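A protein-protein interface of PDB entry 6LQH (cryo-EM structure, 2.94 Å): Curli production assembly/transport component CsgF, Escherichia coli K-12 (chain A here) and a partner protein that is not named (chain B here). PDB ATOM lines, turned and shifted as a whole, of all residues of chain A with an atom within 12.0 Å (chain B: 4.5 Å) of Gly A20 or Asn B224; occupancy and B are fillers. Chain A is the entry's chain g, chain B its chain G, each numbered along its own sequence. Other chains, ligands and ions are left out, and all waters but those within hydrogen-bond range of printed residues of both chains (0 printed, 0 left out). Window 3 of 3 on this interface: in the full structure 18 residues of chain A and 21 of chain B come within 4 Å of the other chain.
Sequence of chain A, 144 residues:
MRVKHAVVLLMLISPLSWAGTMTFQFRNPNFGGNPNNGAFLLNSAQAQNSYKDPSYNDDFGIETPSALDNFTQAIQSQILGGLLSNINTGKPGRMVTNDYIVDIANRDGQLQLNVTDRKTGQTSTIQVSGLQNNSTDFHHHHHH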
ATOM      1  N   GLY A  20       3.224   6.259  25.058  1.00  0.00           N
ATOM      2  CA  GLY A  20       1.908   6.791  25.356  1.00  0.00           C
ATOM      3  C   GLY A  20       0.915   5.706  25.715  1.00  0.00           C
ATOM      4  O   GLY A  20       1.286   4.545  25.862  1.00  0.00           O
ATOM      5  N   THR A  21      -0.352   6.083  25.861  1.00  0.00           N
ATOM      6  CA  THR A  21      -1.379   5.098  26.158  1.00  0.00           C
ATOM      7  C   THR A  21      -1.588   4.166  24.970  1.00  0.00           C
ATOM      8  O   THR A  21      -1.550   4.572  23.806  1.00  0.00           O
ATOM      9  CB  THR A  21      -2.696   5.781  26.548  1.00  0.00           C
ATOM     10  OG1 THR A  21      -3.557   4.839  27.200  1.00  0.00           O
ATOM     11  CG2 THR A  21      -3.410   6.360  25.337  1.00  0.00           C
ATOM     12  N   MET A  22      -1.767   2.890  25.282  1.00  0.00           N
ATOM     13  CA  MET A  22      -2.053   1.863  24.295  1.00  0.00           C
ATOM     14  C   MET A  22      -3.393   1.249  24.640  1.00  0.00           C
ATOM     15  O   MET A  22      -3.629   0.880  25.794  1.00  0.00           O
ATOM     16  CB  MET A  22      -0.962   0.789  24.276  1.00  0.00           C
ATOM     17  CG  MET A  22       0.240   1.144  23.436  1.00  0.00           C
ATOM     18  SD  MET A  22       1.421  -0.201  23.349  1.00  0.00           S
ATOM     19  CE  MET A  22       2.289   0.236  21.859  1.00  0.00           C
ATOM     20  N   THR A  23      -4.271   1.157  23.652  1.00  0.00           N
ATOM     21  CA  THR A  23      -5.602   0.615  23.847  1.00  0.00           C
ATOM     22  C   THR A  23      -5.780  -0.562  22.901  1.00  0.00           C
ATOM     23  O   THR A  23      -5.396  -0.481  21.730  1.00  0.00           O
ATOM     24  CB  THR A  23      -6.662   1.693  23.609  1.00  0.00           C
ATOM     25  OG1 THR A  23      -7.173   2.136  24.869  1.00  0.00           O
ATOM     26  CG2 THR A  23      -7.822   1.159  22.783  1.00  0.00           C
ATOM     27  N   PHE A  24      -6.313  -1.664  23.418  1.00  0.00           N
ATOM     28  CA  PHE A  24      -6.526  -2.840  22.589  1.00  0.00           C
ATOM     29  C   PHE A  24      -7.652  -2.588  21.598  1.00  0.00           C
ATOM     30  O   PHE A  24      -8.725  -2.106  21.971  1.00  0.00           O
ATOM     31  CB  PHE A  24      -6.850  -4.054  23.456  1.00  0.00           C
ATOM     32  CG  PHE A  24      -7.448  -5.200  22.698  1.00  0.00           C
ATOM     33  CD1 PHE A  24      -6.652  -6.047  21.960  1.00  0.00           C
ATOM     34  CD2 PHE A  24      -8.811  -5.432  22.726  1.00  0.00           C
ATOM     35  CE1 PHE A  24      -7.201  -7.095  21.259  1.00  0.00           C
ATOM     36  CE2 PHE A  24      -9.361  -6.482  22.028  1.00  0.00           C
ATOM     37  CZ  PHE A  24      -8.554  -7.315  21.298  1.00  0.00           C
ATOM     38  N   GLN A  25      -7.402  -2.899  20.331  1.00  0.00           N
ATOM     39  CA  GLN A  25      -8.433  -2.901  19.307  1.00  0.00           C
ATOM     40  C   GLN A  25      -8.323  -4.191  18.516  1.00  0.00           C
ATOM     41  O   GLN A  25      -7.217  -4.686  18.277  1.00  0.00           O
ATOM     42  CB  GLN A  25      -8.318  -1.693  18.367  1.00  0.00           C
ATOM     43  CG  GLN A  25      -8.160  -0.344  19.055  1.00  0.00           C
ATOM     44  CD  GLN A  25      -6.799   0.285  18.810  1.00  0.00           C
ATOM     45  OE1 GLN A  25      -6.007  -0.214  18.011  1.00  0.00           O
ATOM     46  NE2 GLN A  25      -6.528   1.393  19.487  1.00  0.00           N
ATOM     47  N   SER B 147       6.799  11.501  25.460  1.00  0.00           N
ATOM     48  CA  SER B 147       5.972  10.420  24.958  1.00  0.00           C
ATOM     49  C   SER B 147       6.739   9.663  23.890  1.00  0.00           C
ATOM     50  O   SER B 147       7.198  10.258  22.912  1.00  0.00           O
ATOM     51  CB  SER B 147       4.660  10.963  24.395  1.00  0.00           C
ATOM     52  OG  SER B 147       3.988   9.987  23.620  1.00  0.00           O
ATOM     53  N   ASN B 148       6.872   8.356  24.083  1.00  0.00           N
ATOM     54  CA  ASN B 148       7.553   7.466  23.147  1.00  0.00           C
ATOM     55  C   ASN B 148       9.016   7.857  22.972  1.00  0.00           C
ATOM     56  O   ASN B 148       9.460   8.222  21.886  1.00  0.00           O
ATOM     57  CB  ASN B 148       6.847   7.440  21.793  1.00  0.00           C
ATOM     58  CG  ASN B 148       5.392   7.098  21.913  1.00  0.00           C
ATOM     59  OD1 ASN B 148       5.015   6.245  22.710  1.00  0.00           O
ATOM     60  ND2 ASN B 148       4.560   7.752  21.117  1.00  0.00           N
ATOM     61  N   GLN B 168       5.966   0.849  23.945  1.00  0.00           N
ATOM     62  CA  GLN B 168       6.291   2.261  23.977  1.00  0.00           C
ATOM     63  C   GLN B 168       6.842   2.577  25.350  1.00  0.00           C
ATOM     64  O   GLN B 168       6.330   2.091  26.356  1.00  0.00           O
ATOM     65  CB  GLN B 168       5.073   3.135  23.703  1.00  0.00           C
ATOM     66  CG  GLN B 168       4.589   3.084  22.284  1.00  0.00           C
ATOM     67  CD  GLN B 168       3.325   3.880  22.082  1.00  0.00           C
ATOM     68  OE1 GLN B 168       2.878   4.587  22.980  1.00  0.00           O
ATOM     69  NE2 GLN B 168       2.739   3.769  20.900  1.00  0.00           N
ATOM     70  N   ASP B 170       7.400   5.834  27.614  1.00  0.00           N
ATOM     71  CA  ASP B 170       7.406   7.247  27.929  1.00  0.00           C
ATOM     72  C   ASP B 170       8.448   7.488  29.009  1.00  0.00           C
ATOM     73  O   ASP B 170       9.001   6.555  29.583  1.00  0.00           O
ATOM     74  CB  ASP B 170       6.029   7.723  28.374  1.00  0.00           C
ATOM     75  CG  ASP B 170       4.950   7.398  27.373  1.00  0.00           C
ATOM     76  OD1 ASP B 170       5.224   7.446  26.157  1.00  0.00           O
ATOM     77  OD2 ASP B 170       3.816   7.109  27.803  1.00  0.00           O
ATOM     78  N   LEU B 197       6.433   1.994  30.722  1.00  0.00           N
ATOM     79  CA  LEU B 197       6.314   1.009  29.658  1.00  0.00           C
ATOM     80  C   LEU B 197       4.852   0.722  29.358  1.00  0.00           C
ATOM     81  O   LEU B 197       4.056   0.493  30.267  1.00  0.00           O
ATOM     82  CB  LEU B 197       7.023  -0.284  30.040  1.00  0.00           C
ATOM     83  CG  LEU B 197       6.795  -1.434  29.063  1.00  0.00           C
ATOM     84  CD1 LEU B 197       7.601  -1.243  27.800  1.00  0.00           C
ATOM     85  CD2 LEU B 197       7.125  -2.751  29.716  1.00  0.00           C
ATOM     86  N   SER B 198       4.503   0.719  28.079  1.00  0.00           N
ATOM     87  CA  SER B 198       3.161   0.383  27.615  1.00  0.00           C
ATOM     88  C   SER B 198       3.328  -0.624  26.491  1.00  0.00           C
ATOM     89  O   SER B 198       3.786  -0.260  25.413  1.00  0.00           O
ATOM     90  CB  SER B 198       2.419   1.614  27.116  1.00  0.00           C
ATOM     91  OG  SER B 198       2.885   2.793  27.745  1.00  0.00           O
ATOM     92  N   THR B 222      -3.159  -5.738  26.355  1.00  0.00           N
ATOM     93  CA  THR B 222      -2.473  -4.460  26.395  1.00  0.00           C
ATOM     94  C   THR B 222      -2.187  -4.129  27.846  1.00  0.00           C
ATOM     95  O   THR B 222      -2.936  -4.541  28.734  1.00  0.00           O
ATOM     96  CB  THR B 222      -3.307  -3.361  25.744  1.00  0.00           C
ATOM     97  OG1 THR B 222      -3.845  -3.850  24.520  1.00  0.00           O
ATOM     98  CG2 THR B 222      -2.468  -2.151  25.456  1.00  0.00           C
ATOM     99  N   SER B 223      -1.095  -3.414  28.092  1.00  0.00           N
ATOM    100  CA  SER B 223      -0.726  -3.017  29.444  1.00  0.00           C
ATOM    101  C   SER B 223      -0.070  -1.652  29.377  1.00  0.00           C
ATOM    102  O   SER B 223       1.044  -1.525  28.868  1.00  0.00           O
ATOM    103  CB  SER B 223       0.201  -4.048  30.078  1.00  0.00           C
ATOM    104  OG  SER B 223       0.588  -3.653  31.382  1.00  0.00           O
ATOM    105  N   ASN B 224      -0.765  -0.639  29.872  1.00  0.00           N
ATOM    106  CA  ASN B 224      -0.207   0.693  30.017  1.00  0.00           C
ATOM    107  C   ASN B 224       0.179   0.911  31.470  1.00  0.00           C
ATOM    108  O   ASN B 224      -0.674   0.837  32.355  1.00  0.00           O
ATOM    109  CB  ASN B 224      -1.211   1.757  29.582  1.00  0.00           C
ATOM    110  CG  ASN B 224      -1.618   1.610  28.145  1.00  0.00           C
ATOM    111  OD1 ASN B 224      -0.881   1.990  27.243  1.00  0.00           O
ATOM    112  ND2 ASN B 224      -2.798   1.061  27.916  1.00  0.00           N
ATOM    113  N   GLU B 225       1.457   1.156  31.717  1.00  0.00           N
ATOM    114  CA  GLU B 225       1.873   1.467  33.072  1.00  0.00           C
ATOM    115  C   GLU B 225       1.271   2.804  33.481  1.00  0.00           C
ATOM    116  O   GLU B 225       1.402   3.788  32.750  1.00  0.00           O
ATOM    117  CB  GLU B 225       3.391   1.519  33.191  1.00  0.00           C
ATOM    118  CG  GLU B 225       4.015   0.206  33.624  1.00  0.00           C
ATOM    119  CD  GLU B 225       5.451   0.362  34.070  1.00  0.00           C
ATOM    120  OE1 GLU B 225       5.848   1.498  34.400  1.00  0.00           O
ATOM    121  OE2 GLU B 225       6.184  -0.649  34.085  1.00  0.00           O
ATOM    122  N   PRO B 226       0.581   2.868  34.614  1.00  0.00           N
ATOM    123  CA  PRO B 226      -0.044   4.128  35.013  1.00  0.00           C
ATOM    124  C   PRO B 226       0.984   5.230  35.194  1.00  0.00           C
ATOM    125  O   PRO B 226       2.026   5.037  35.821  1.00  0.00           O
ATOM    126  CB  PRO B 226      -0.733   3.778  36.336  1.00  0.00           C
ATOM    127  CG  PRO B 226      -0.927   2.315  36.275  1.00  0.00           C
ATOM    128  CD  PRO B 226       0.264   1.784  35.554  1.00  0.00           C
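Gly A20 touches just these residues of chain B: Asn B148, Gln B168, Asp B170, Ser B198 and Asn B224. Asn B224 touches just these residues of chain A: Gly A20 (3.6 Å), Thr A21 (3.2 Å) and Met A22 (2.3 Å). Of chain A, only Gly A20 (3.0 Å) comes within 4 Å of Asn B148. Of chain A, only Gly A20 and Met A22 come within 4 Å of Gln B168. Asp B170 touches just one residue of chain A: Gly A20. Printed residues of chain A within 4 Å of Thr B222: Met A22 and Phe A24. No residue of chain A comes within 4 Å of Ser B223. No residue of chain A comes within 4 Å of Glu B225. Printed residues of chain B within 4 Å of Phe A24: Thr B222 (3.2 Å). Of the printed residues of chain B, Met A22 touches Gln B168 (3.7 Å), Ser B198 (3.1 Å), Thr B222 (3.3 Å) and Asn B224 (2.3 Å). Printed residues of chain B within 4 Å of Thr A21: Asn B224 (3.2 Å). Thr A23 touches none of the printed residues of chain B. The nearest residue of chain A that does not touch Asn B224 is Thr A23 (4.5 Å). The nearest printed residue of chain B that does not touch Met A22 is Ser B223 (5.5 Å).
The side-chain hydroxyl (OG) of Ser B147 sits at hydrogen-bond distance from the side-chain amide nitrogen (ND2) of Asn B148 (3.4 Å). OE1 of Gln B168 lies close to OD1 of Asn B148 (2.7 Å). The backbone NH of Asn B148 lies within hydrogen-bond range of the side-chain carboxylate of Asp B170, at 2.8 Å. N of Gln B168 sits at hydrogen-bond distance from O of Ser B198 (2.9 Å).
O of Gly A20 touches OD1 of Asn B224, 3.6 Å away. Asn B224 touches Thr A21. Met A22 touches Gln B168. Thr B222 touches Met A22 (CG2 to O, 3.3 Å).
The side-chain amide oxygen (OD1) of Asn B148 lies within hydrogen-bond range of the backbone NH (N) of Gly A20. OE1 of Gln B168 is in hydrogen-bond range of N of Gly A20. The side-chain carboxylate (OD1) of Asp B170 is in hydrogen-bond range of the backbone NH (N) of Gly A20 (2.6 Å). The side-chain hydroxyl (OG) of Ser B198 lies within hydrogen-bond range of the backbone carbonyl oxygen (O) of Gly A20 (3.0 Å). The backbone NH (N) of Phe A24 lies close to the side-chain hydroxyl (OG1) of Thr B222 (3.5 Å). OD1 of Asn B224 lies close to O of Met A22, at 3.3 Å. The side-chain sulfur of Met A22 sits close to the backbone carbonyl oxygen of Ser B198 (3.1 Å).
Printed residues of chain A that touch a printed residue of chain B: Gly A20, Thr A21, Met A22 and Phe A24. Of the 11 printed residues of chain B, 6 touch a printed residue of chain A. Along chain B the printed residues that touch a printed residue of chain A span positions 148 to 224. Among the printed residues, 11 pairs touch across the chains.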
